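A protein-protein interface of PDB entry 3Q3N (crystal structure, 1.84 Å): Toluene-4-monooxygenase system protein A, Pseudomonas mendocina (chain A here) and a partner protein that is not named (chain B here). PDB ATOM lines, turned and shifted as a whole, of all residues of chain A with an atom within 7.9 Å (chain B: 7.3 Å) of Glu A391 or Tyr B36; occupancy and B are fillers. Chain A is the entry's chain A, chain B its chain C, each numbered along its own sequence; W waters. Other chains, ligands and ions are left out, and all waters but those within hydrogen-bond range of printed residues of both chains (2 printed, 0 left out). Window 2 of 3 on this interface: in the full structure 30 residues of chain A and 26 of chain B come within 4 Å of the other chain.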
ATOM      1  N   TYR A 337     -34.685 -26.192 -12.097  1.00  0.00           N
ATOM      2  CA  TYR A 337     -33.685 -27.144 -11.625  1.00  0.00           C
ATOM      3  C   TYR A 337     -33.952 -27.518 -10.168  1.00  0.00           C
ATOM      4  O   TYR A 337     -33.823 -28.682  -9.789  1.00  0.00           O
ATOM      5  CB  TYR A 337     -32.249 -26.614 -11.794  1.00  0.00           C
ATOM      6  CG  TYR A 337     -31.232 -27.739 -11.770  1.00  0.00           C
ATOM      7  CD1 TYR A 337     -30.945 -28.468 -12.922  1.00  0.00           C
ATOM      8  CD2 TYR A 337     -30.598 -28.103 -10.592  1.00  0.00           C
ATOM      9  CE1 TYR A 337     -30.027 -29.509 -12.903  1.00  0.00           C
ATOM     10  CE2 TYR A 337     -29.681 -29.140 -10.564  1.00  0.00           C
ATOM     11  CZ  TYR A 337     -29.407 -29.842 -11.722  1.00  0.00           C
ATOM     12  OH  TYR A 337     -28.501 -30.874 -11.702  1.00  0.00           O
ATOM     13  N   TRP A 338     -34.344 -26.531  -9.365  1.00  0.00           N
ATOM     14  CA  TRP A 338     -34.687 -26.758  -7.961  1.00  0.00           C
ATOM     15  C   TRP A 338     -36.200 -26.872  -7.776  1.00  0.00           C
ATOM     16  O   TRP A 338     -36.735 -26.503  -6.729  1.00  0.00           O
ATOM     17  CB  TRP A 338     -34.120 -25.638  -7.071  1.00  0.00           C
ATOM     18  CG  TRP A 338     -32.660 -25.834  -6.713  1.00  0.00           C
ATOM     19  CD1 TRP A 338     -32.160 -26.348  -5.549  1.00  0.00           C
ATOM     20  CD2 TRP A 338     -31.526 -25.508  -7.526  1.00  0.00           C
ATOM     21  NE1 TRP A 338     -30.786 -26.376  -5.595  1.00  0.00           N
ATOM     22  CE2 TRP A 338     -30.371 -25.862  -6.795  1.00  0.00           C
ATOM     23  CE3 TRP A 338     -31.376 -24.951  -8.803  1.00  0.00           C
ATOM     24  CZ2 TRP A 338     -29.085 -25.686  -7.300  1.00  0.00           C
ATOM     25  CZ3 TRP A 338     -30.095 -24.775  -9.303  1.00  0.00           C
ATOM     26  CH2 TRP A 338     -28.965 -25.140  -8.548  1.00  0.00           C
ATOM     27  N   MET A 385     -31.217 -39.178 -14.882  1.00  0.00           N
ATOM     28  CA  MET A 385     -32.083 -38.261 -14.147  1.00  0.00           C
ATOM     29  C   MET A 385     -31.436 -37.687 -12.891  1.00  0.00           C
ATOM     30  O   MET A 385     -31.823 -36.622 -12.417  1.00  0.00           O
ATOM     31  CB  MET A 385     -33.426 -38.918 -13.825  1.00  0.00           C
ATOM     32  CG  MET A 385     -34.185 -39.391 -15.061  1.00  0.00           C
ATOM     33  SD  MET A 385     -34.393 -38.089 -16.291  1.00  0.00           S
ATOM     34  CE  MET A 385     -35.584 -37.048 -15.456  1.00  0.00           C
ATOM     35  N   ASP A 386     -30.432 -38.370 -12.358  1.00  0.00           N
ATOM     36  CA  ASP A 386     -29.749 -37.831 -11.189  1.00  0.00           C
ATOM     37  C   ASP A 386     -29.075 -36.495 -11.501  1.00  0.00           C
ATOM     38  O   ASP A 386     -28.860 -35.685 -10.605  1.00  0.00           O
ATOM     39  CB  ASP A 386     -28.726 -38.828 -10.647  1.00  0.00           C
ATOM     40  CG  ASP A 386     -27.711 -39.229 -11.683  1.00  0.00           C
ATOM     41  OD1 ASP A 386     -26.504 -39.074 -11.414  1.00  0.00           O
ATOM     42  OD2 ASP A 386     -28.122 -39.699 -12.766  1.00  0.00           O
ATOM     43  N   LEU A 387     -28.739 -36.270 -12.770  1.00  0.00           N
ATOM     44  CA  LEU A 387     -28.055 -35.037 -13.182  1.00  0.00           C
ATOM     45  C   LEU A 387     -29.034 -33.883 -13.420  1.00  0.00           C
ATOM     46  O   LEU A 387     -28.626 -32.759 -13.741  1.00  0.00           O
ATOM     47  CB  LEU A 387     -27.206 -35.282 -14.434  1.00  0.00           C
ATOM     48  CG  LEU A 387     -26.071 -36.299 -14.257  1.00  0.00           C
ATOM     49  CD1 LEU A 387     -25.295 -36.523 -15.552  1.00  0.00           C
ATOM     50  CD2 LEU A 387     -25.134 -35.833 -13.151  1.00  0.00           C
ATOM     51  N   VAL A 388     -30.323 -34.159 -13.248  1.00  0.00           N
ATOM     52  CA  VAL A 388     -31.348 -33.132 -13.418  1.00  0.00           C
ATOM     53  C   VAL A 388     -32.016 -32.791 -12.087  1.00  0.00           C
ATOM     54  O   VAL A 388     -33.110 -32.223 -12.052  1.00  0.00           O
ATOM     55  CB  VAL A 388     -32.408 -33.551 -14.453  1.00  0.00           C
ATOM     56  CG1 VAL A 388     -31.742 -33.925 -15.766  1.00  0.00           C
ATOM     57  CG2 VAL A 388     -33.230 -34.711 -13.932  1.00  0.00           C
ATOM     58  N   SER A 389     -31.346 -33.151 -10.995  1.00  0.00           N
ATOM     59  CA  SER A 389     -31.777 -32.770  -9.655  1.00  0.00           C
ATOM     60  C   SER A 389     -30.583 -32.341  -8.807  1.00  0.00           C
ATOM     61  O   SER A 389     -29.526 -32.972  -8.848  1.00  0.00           O
ATOM     62  CB  SER A 389     -32.522 -33.911  -8.980  1.00  0.00           C
ATOM     63  OG  SER A 389     -33.727 -34.170  -9.667  1.00  0.00           O
ATOM     64  N   PRO A 390     -30.754 -31.266  -8.027  1.00  0.00           N
ATOM     65  CA  PRO A 390     -29.630 -30.650  -7.316  1.00  0.00           C
ATOM     66  C   PRO A 390     -29.197 -31.425  -6.074  1.00  0.00           C
ATOM     67  O   PRO A 390     -29.995 -32.131  -5.459  1.00  0.00           O
ATOM     68  CB  PRO A 390     -30.196 -29.293  -6.905  1.00  0.00           C
ATOM     69  CG  PRO A 390     -31.657 -29.577  -6.693  1.00  0.00           C
ATOM     70  CD  PRO A 390     -32.034 -30.589  -7.742  1.00  0.00           C
ATOM     71  N   GLU A 391     -27.936 -31.268  -5.703  1.00  0.00           N
ATOM     72  CA  GLU A 391     -27.418 -31.870  -4.485  1.00  0.00           C
ATOM     73  C   GLU A 391     -26.785 -30.804  -3.600  1.00  0.00           C
ATOM     74  O   GLU A 391     -25.979 -31.102  -2.720  1.00  0.00           O
ATOM     75  CB  GLU A 391     -26.427 -32.980  -4.829  1.00  0.00           C
ATOM     76  CG  GLU A 391     -27.084 -34.130  -5.589  1.00  0.00           C
ATOM     77  CD  GLU A 391     -26.084 -35.148  -6.106  1.00  0.00           C
ATOM     78  OE1 GLU A 391     -25.066 -35.396  -5.424  1.00  0.00           O
ATOM     79  OE2 GLU A 391     -26.320 -35.697  -7.203  1.00  0.00           O
ATOM     80  N   THR A 392     -27.155 -29.553  -3.847  1.00  0.00           N
ATOM     81  CA  THR A 392     -26.703 -28.442  -3.008  1.00  0.00           C
ATOM     82  C   THR A 392     -27.654 -27.261  -3.130  1.00  0.00           C
ATOM     83  O   THR A 392     -28.556 -27.286  -3.965  1.00  0.00           O
ATOM     84  CB  THR A 392     -25.267 -27.994  -3.354  1.00  0.00           C
ATOM     85  OG1 THR A 392     -24.789 -27.106  -2.335  1.00  0.00           O
ATOM     86  CG2 THR A 392     -25.229 -27.279  -4.706  1.00  0.00           C
ATOM     87  N   LEU A 393     -27.449 -26.236  -2.300  1.00  0.00           N
ATOM     88  CA  LEU A 393     -28.283 -25.036  -2.316  1.00  0.00           C
ATOM     89  C   LEU A 393     -27.752 -24.012  -3.311  1.00  0.00           C
ATOM     90  O   LEU A 393     -26.549 -23.925  -3.536  1.00  0.00           O
ATOM     91  CB  LEU A 393     -28.297 -24.376  -0.937  1.00  0.00           C
ATOM     92  CG  LEU A 393     -28.956 -25.064   0.252  1.00  0.00           C
ATOM     93  CD1 LEU A 393     -28.563 -24.355   1.531  1.00  0.00           C
ATOM     94  CD2 LEU A 393     -30.430 -25.035   0.094  1.00  0.00           C
ATOM     95  N   PRO A 394     -28.651 -23.233  -3.915  1.00  0.00           N
ATOM     96  CA  PRO A 394     -28.154 -22.078  -4.658  1.00  0.00           C
ATOM     97  C   PRO A 394     -27.772 -20.992  -3.672  1.00  0.00           C
ATOM     98  O   PRO A 394     -28.323 -20.968  -2.568  1.00  0.00           O
ATOM     99  CB  PRO A 394     -29.374 -21.640  -5.475  1.00  0.00           C
ATOM    100  CG  PRO A 394     -30.542 -22.125  -4.704  1.00  0.00           C
ATOM    101  CD  PRO A 394     -30.118 -23.373  -4.000  1.00  0.00           C
ATOM    102  N   THR A 463     -29.807 -31.316   4.975  1.00  0.00           N
ATOM    103  CA  THR A 463     -29.920 -32.148   3.782  1.00  0.00           C
ATOM    104  C   THR A 463     -31.094 -31.627   2.980  1.00  0.00           C
ATOM    105  O   THR A 463     -31.829 -30.764   3.452  1.00  0.00           O
ATOM    106  CB  THR A 463     -30.263 -33.597   4.127  1.00  0.00           C
ATOM    107  OG1 THR A 463     -31.495 -33.622   4.858  1.00  0.00           O
ATOM    108  CG2 THR A 463     -29.152 -34.264   4.954  1.00  0.00           C
ATOM    109  N   LEU A 464     -31.295 -32.173   1.786  1.00  0.00           N
ATOM    110  CA  LEU A 464     -32.416 -31.741   0.960  1.00  0.00           C
ATOM    111  C   LEU A 464     -33.737 -32.010   1.677  1.00  0.00           C
ATOM    112  O   LEU A 464     -34.628 -31.165   1.678  1.00  0.00           O
ATOM    113  CB  LEU A 464     -32.392 -32.423  -0.412  1.00  0.00           C
ATOM    114  CG  LEU A 464     -33.534 -32.069  -1.378  1.00  0.00           C
ATOM    115  CD1 LEU A 464     -33.580 -30.576  -1.655  1.00  0.00           C
ATOM    116  CD2 LEU A 464     -33.386 -32.850  -2.672  1.00  0.00           C
ATOM    117  N   PHE B  10     -19.403 -21.239 -11.468  1.00  0.00           N
ATOM    118  CA  PHE B  10     -18.634 -22.014 -12.429  1.00  0.00           C
ATOM    119  C   PHE B  10     -18.776 -21.430 -13.831  1.00  0.00           C
ATOM    120  O   PHE B  10     -19.865 -21.021 -14.227  1.00  0.00           O
ATOM    121  CB  PHE B  10     -19.068 -23.480 -12.423  1.00  0.00           C
ATOM    122  CG  PHE B  10     -18.134 -24.388 -13.164  1.00  0.00           C
ATOM    123  CD1 PHE B  10     -18.241 -24.542 -14.537  1.00  0.00           C
ATOM    124  CD2 PHE B  10     -17.140 -25.079 -12.489  1.00  0.00           C
ATOM    125  CE1 PHE B  10     -17.377 -25.379 -15.225  1.00  0.00           C
ATOM    126  CE2 PHE B  10     -16.272 -25.918 -13.166  1.00  0.00           C
ATOM    127  CZ  PHE B  10     -16.389 -26.069 -14.536  1.00  0.00           C
ATOM    128  N   GLN B  17     -23.543 -21.048  -6.540  1.00  0.00           N
ATOM    129  CA  GLN B  17     -24.061 -22.077  -5.631  1.00  0.00           C
ATOM    130  C   GLN B  17     -23.269 -22.158  -4.334  1.00  0.00           C
ATOM    131  O   GLN B  17     -22.088 -21.795  -4.296  1.00  0.00           O
ATOM    132  CB  GLN B  17     -24.034 -23.457  -6.290  1.00  0.00           C
ATOM    133  CG  GLN B  17     -25.066 -23.687  -7.360  1.00  0.00           C
ATOM    134  CD  GLN B  17     -24.788 -24.971  -8.106  1.00  0.00           C
ATOM    135  OE1 GLN B  17     -23.680 -25.182  -8.607  1.00  0.00           O
ATOM    136  NE2 GLN B  17     -25.772 -25.856  -8.150  1.00  0.00           N
ATOM    137  N   LEU B  18     -23.916 -22.653  -3.280  1.00  0.00           N
ATOM    138  CA  LEU B  18     -23.210 -22.981  -2.043  1.00  0.00           C
ATOM    139  C   LEU B  18     -22.454 -24.294  -2.211  1.00  0.00           C
ATOM    140  O   LEU B  18     -23.043 -25.320  -2.534  1.00  0.00           O
ATOM    141  CB  LEU B  18     -24.178 -23.103  -0.864  1.00  0.00           C
ATOM    142  CG  LEU B  18     -23.535 -23.637   0.421  1.00  0.00           C
ATOM    143  CD1 LEU B  18     -22.617 -22.579   1.058  1.00  0.00           C
ATOM    144  CD2 LEU B  18     -24.595 -24.109   1.412  1.00  0.00           C
ATOM    145  N   VAL B  30     -10.881 -27.943  -4.656  1.00  0.00           N
ATOM    146  CA  VAL B  30     -12.022 -27.046  -4.595  1.00  0.00           C
ATOM    147  C   VAL B  30     -12.673 -26.973  -5.969  1.00  0.00           C
ATOM    148  O   VAL B  30     -13.897 -26.977  -6.086  1.00  0.00           O
ATOM    149  CB  VAL B  30     -11.594 -25.628  -4.169  1.00  0.00           C
ATOM    150  CG1 VAL B  30     -12.779 -24.673  -4.216  1.00  0.00           C
ATOM    151  CG2 VAL B  30     -10.971 -25.651  -2.782  1.00  0.00           C
ATOM    152  N   ALA B  31     -11.843 -26.905  -7.007  1.00  0.00           N
ATOM    153  CA  ALA B  31     -12.325 -26.745  -8.375  1.00  0.00           C
ATOM    154  C   ALA B  31     -13.100 -27.980  -8.784  1.00  0.00           C
ATOM    155  O   ALA B  31     -14.049 -27.908  -9.570  1.00  0.00           O
ATOM    156  CB  ALA B  31     -11.159 -26.512  -9.325  1.00  0.00           C
ATOM    157  N   GLU B  32     -12.686 -29.112  -8.227  1.00  0.00           N
ATOM    158  CA  GLU B  32     -13.331 -30.385  -8.485  1.00  0.00           C
ATOM    159  C   GLU B  32     -14.688 -30.450  -7.795  1.00  0.00           C
ATOM    160  O   GLU B  32     -15.671 -30.911  -8.381  1.00  0.00           O
ATOM    161  CB  GLU B  32     -12.445 -31.530  -7.994  1.00  0.00           C
ATOM    162  CG  GLU B  32     -12.775 -32.851  -8.639  1.00  0.00           C
ATOM    163  CD  GLU B  32     -12.562 -32.810 -10.135  1.00  0.00           C
ATOM    164  OE1 GLU B  32     -11.459 -32.404 -10.566  1.00  0.00           O
ATOM    165  OE2 GLU B  32     -13.498 -33.172 -10.878  1.00  0.00           O
ATOM    166  N   LYS B  33     -14.741 -29.980  -6.551  1.00  0.00           N
ATOM    167  CA  LYS B  33     -15.967 -30.046  -5.758  1.00  0.00           C
ATOM    168  C   LYS B  33     -17.045 -29.127  -6.309  1.00  0.00           C
ATOM    169  O   LYS B  33     -18.235 -29.420  -6.206  1.00  0.00           O
ATOM    170  CB  LYS B  33     -15.688 -29.724  -4.291  1.00  0.00           C
ATOM    171  CG  LYS B  33     -14.815 -30.764  -3.611  1.00  0.00           C
ATOM    172  CD  LYS B  33     -14.590 -30.454  -2.147  1.00  0.00           C
ATOM    173  CE  LYS B  33     -13.796 -31.575  -1.482  1.00  0.00           C
ATOM    174  NZ  LYS B  33     -13.574 -31.310  -0.039  1.00  0.00           N
ATOM    175  N   VAL B  34     -16.622 -28.011  -6.887  1.00  0.00           N
ATOM    176  CA  VAL B  34     -17.548 -27.118  -7.563  1.00  0.00           C
ATOM    177  C   VAL B  34     -18.028 -27.766  -8.857  1.00  0.00           C
ATOM    178  O   VAL B  34     -19.231 -27.874  -9.101  1.00  0.00           O
ATOM    179  CB  VAL B  34     -16.898 -25.763  -7.881  1.00  0.00           C
ATOM    180  CG1 VAL B  34     -17.863 -24.886  -8.673  1.00  0.00           C
ATOM    181  CG2 VAL B  34     -16.460 -25.069  -6.596  1.00  0.00           C
ATOM    182  N   ALA B  35     -17.084 -28.206  -9.684  1.00  0.00           N
ATOM    183  CA  ALA B  35     -17.421 -28.834 -10.958  1.00  0.00           C
ATOM    184  C   ALA B  35     -18.485 -29.919 -10.783  1.00  0.00           C
ATOM    185  O   ALA B  35     -19.365 -30.093 -11.636  1.00  0.00           O
ATOM    186  CB  ALA B  35     -16.172 -29.411 -11.610  1.00  0.00           C
ATOM    187  N   TYR B  36     -18.410 -30.642  -9.671  1.00  0.00           N
ATOM    188  CA  TYR B  36     -19.354 -31.721  -9.426  1.00  0.00           C
ATOM    189  C   TYR B  36     -20.792 -31.254  -9.580  1.00  0.00           C
ATOM    190  O   TYR B  36     -21.656 -31.997 -10.069  1.00  0.00           O
ATOM    191  CB  TYR B  36     -19.163 -32.318  -8.030  1.00  0.00           C
ATOM    192  CG  TYR B  36     -20.175 -33.397  -7.727  1.00  0.00           C
ATOM    193  CD1 TYR B  36     -19.939 -34.719  -8.096  1.00  0.00           C
ATOM    194  CD2 TYR B  36     -21.383 -33.092  -7.102  1.00  0.00           C
ATOM    195  CE1 TYR B  36     -20.870 -35.715  -7.836  1.00  0.00           C
ATOM    196  CE2 TYR B  36     -22.316 -34.078  -6.837  1.00  0.00           C
ATOM    197  CZ  TYR B  36     -22.054 -35.388  -7.208  1.00  0.00           C
ATOM    198  OH  TYR B  36     -22.974 -36.377  -6.951  1.00  0.00           O
ATOM    199  N   HIS B  37     -21.056 -30.023  -9.158  1.00  0.00           N
ATOM    200  CA  HIS B  37     -22.428 -29.539  -9.133  1.00  0.00           C
ATOM    201  C   HIS B  37     -22.784 -28.767 -10.395  1.00  0.00           C
ATOM    202  O   HIS B  37     -23.817 -28.109 -10.437  1.00  0.00           O
ATOM    203  CB  HIS B  37     -22.669 -28.654  -7.903  1.00  0.00           C
ATOM    204  CG  HIS B  37     -22.514 -29.368  -6.594  1.00  0.00           C
ATOM    205  ND1 HIS B  37     -23.472 -30.224  -6.095  1.00  0.00           N
ATOM    206  CD2 HIS B  37     -21.518 -29.341  -5.677  1.00  0.00           C
ATOM    207  CE1 HIS B  37     -23.071 -30.698  -4.929  1.00  0.00           C
ATOM    208  NE2 HIS B  37     -21.887 -30.180  -4.653  1.00  0.00           N
ATOM    209  N   CYS B  38     -21.931 -28.843 -11.415  1.00  0.00           N
ATOM    210  CA  CYS B  38     -22.064 -27.974 -12.587  1.00  0.00           C
ATOM    211  C   CYS B  38     -21.851 -28.696 -13.916  1.00  0.00           C
ATOM    212  O   CYS B  38     -22.744 -28.719 -14.771  1.00  0.00           O
ATOM    213  CB  CYS B  38     -21.090 -26.797 -12.478  1.00  0.00           C
ATOM    214  SG  CYS B  38     -21.256 -25.852 -10.948  1.00  0.00           S
ATOM    215  N   VAL B  39     -20.658 -29.262 -14.095  1.00  0.00           N
ATOM    216  CA  VAL B  39     -20.333 -29.999 -15.309  1.00  0.00           C
ATOM    217  C   VAL B  39     -21.240 -31.224 -15.431  1.00  0.00           C
ATOM    218  O   VAL B  39     -21.458 -31.940 -14.452  1.00  0.00           O
ATOM    219  CB  VAL B  39     -18.854 -30.440 -15.327  1.00  0.00           C
ATOM    220  CG1 VAL B  39     -18.564 -31.289 -16.558  1.00  0.00           C
ATOM    221  CG2 VAL B  39     -17.929 -29.220 -15.271  1.00  0.00           C
ATOM    222  N   ASN B  40     -21.770 -31.447 -16.631  1.00  0.00           N
ATOM    223  CA  ASN B  40     -22.688 -32.555 -16.894  1.00  0.00           C
ATOM    224  C   ASN B  40     -24.068 -32.364 -16.273  1.00  0.00           C
ATOM    225  O   ASN B  40     -24.878 -33.286 -16.250  1.00  0.00           O
ATOM    226  CB  ASN B  40     -22.084 -33.898 -16.464  1.00  0.00           C
ATOM    227  CG  ASN B  40     -20.977 -34.357 -17.388  1.00  0.00           C
ATOM    228  OD1 ASN B  40     -20.996 -34.066 -18.584  1.00  0.00           O
ATOM    229  ND2 ASN B  40     -20.004 -35.075 -16.840  1.00  0.00           N
ATOM    230  N   ARG B  41     -24.319 -31.165 -15.760  1.00  0.00           N
ATOM    231  CA  ARG B  41     -25.641 -30.792 -15.274  1.00  0.00           C
ATOM    232  C   ARG B  41     -26.166 -29.627 -16.088  1.00  0.00           C
ATOM    233  O   ARG B  41     -27.241 -29.707 -16.676  1.00  0.00           O
ATOM    234  CB  ARG B  41     -25.603 -30.427 -13.789  1.00  0.00           C
ATOM    235  CG  ARG B  41     -25.246 -31.610 -12.895  1.00  0.00           C
ATOM    236  CD  ARG B  41     -25.230 -31.230 -11.426  1.00  0.00           C
ATOM    237  NE  ARG B  41     -24.809 -32.356 -10.601  1.00  0.00           N
ATOM    238  CZ  ARG B  41     -25.643 -33.168  -9.961  1.00  0.00           C
ATOM    239  NH1 ARG B  41     -26.954 -32.972 -10.034  1.00  0.00           N
ATOM    240  NH2 ARG B  41     -25.165 -34.177  -9.244  1.00  0.00           N
ATOM    241  N   MET B  50      -8.883 -26.592 -14.639  1.00  0.00           N
ATOM    242  CA  MET B  50      -9.779 -25.755 -13.853  1.00  0.00           C
ATOM    243  C   MET B  50      -8.995 -24.954 -12.828  1.00  0.00           C
ATOM    244  O   MET B  50      -8.168 -25.505 -12.099  1.00  0.00           O
ATOM    245  CB  MET B  50     -10.836 -26.603 -13.151  1.00  0.00           C
ATOM    246  CG  MET B  50     -11.923 -27.115 -14.067  1.00  0.00           C
ATOM    247  SD  MET B  50     -13.216 -27.995 -13.174  1.00  0.00           S
ATOM    248  CE  MET B  50     -12.280 -29.327 -12.417  1.00  0.00           C
HETATM  249  O   HOH W   1     -26.014 -30.413  -7.637  1.00  0.00           O
HETATM  250  O   HOH W   2     -28.887 -31.833 -16.470  1.00  0.00           O
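OH of Tyr A337 lies within hydrogen-bond range of NH1 of Arg B41, 3.1 Å away. The guanidinium group of Arg B41 lies within hydrogen-bond range of the backbone carbonyl oxygen of Asp A386 (3.4 Å). O of Ser A389 lies within hydrogen-bond range of NH1 of Arg B41, at 2.8 Å. The side-chain carboxylate (OE1) of Glu A391 lies within hydrogen-bond range of the side-chain hydroxyl (OH) of Tyr B36 (2.8 Å). OE2 of Glu A391 is in salt-bridge range of NH2 of Arg B41 (2.8 Å). The side-chain hydroxyl (OG1) of Thr A392 is in hydrogen-bond range of the backbone carbonyl oxygen (O) of Leu B18, at 2.5 Å. O of Leu A393 sits at hydrogen-bond distance from N of Leu B18, 2.9 Å away.
Glu A391 touches just these residues of chain B: Tyr B36, His B37 and Arg B41. Of chain A, only Glu A391 (2.8 Å) comes within 4 Å of Tyr B36. Printed residues of chain A within 4 Å of His B37: Glu A391 (3.7 Å) and Thr A392 (3.7 Å). Of the printed residues of chain B, Tyr A337 touches Arg B41 (3.1 Å). Of the printed residues of chain B, Ser A389 touches Arg B41 (2.8 Å). Printed residues of chain A within 4 Å of Leu B18: Thr A392 and Leu A393. Val B39 touches none of the printed residues of chain A. Val A388 touches none of the printed residues of chain B. The nearest residue of chain B that does not touch Glu A391 is Gln B17 (6.3 Å). The nearest printed residue of chain A that does not touch Leu B18 is Pro A394 (4.2 Å).
The backbone carbonyl oxygen of Leu A387 is in hydrogen-bond range of the side-chain hydroxyl of Tyr A337, at 2.8 Å. NE1 of Trp A338 sits at hydrogen-bond distance from O of Thr A392 (2.9 Å). OE1 of Gln B17 lies close to O of His B37, at 3.5 Å. The side-chain amide oxygen of Gln B17 sits at hydrogen-bond distance from the side-chain sulfur of Cys B38 (3.4 Å). The backbone carbonyl oxygen (O) of Tyr B36 sits at hydrogen-bond distance from the guanidinium group (NE) of Arg B41.
Printed residues of chain B that touch a printed residue of chain A: Gln B17, Leu B18, Tyr B36, His B37, Asn B40 and Arg B41. Hydrophobic or aromatic side chains of chain B within 4 Å of the printed part of chain A: Leu B18, Tyr B36 and His B37. Of the 14 printed residues of chain A, 8 touch a printed residue of chain B. Hydrophobic or aromatic side chains of chain A within 4 Å of the printed part of chain B: Tyr A337, Trp A338, Leu A387 and Leu A393. Among the printed residues, Asp or Glu carboxylates within 4 Å of a Lys or Arg side-chain nitrogen of the other chain: Glu A391 with Arg B41.
Among the printed residues, merely in contact across the chains: Trp A338 with Gln B17 (3.3 Å), Leu A387 with Asn B40 (3.3 Å), Leu A387 with Arg B41 (3.7 Å), Glu A391 with His B37 (3.7 Å), Thr A392 with Gln B17 (3.8 Å), Thr A392 with His B37 (3.7 Å) and Leu A393 with Gln B17 (3.7 Å).
Water W2 bridges the backbone carbonyl oxygen (O) of Arg B41 (2.7 Å) and the backbone carbonyl oxygen (O) of Leu A387 (2.9 Å). Water W1 lies within hydrogen-bond range of the backbone NH of Glu A391 (2.9 Å) and a ring nitrogen (ND1) of His B37 (3.0 Å).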
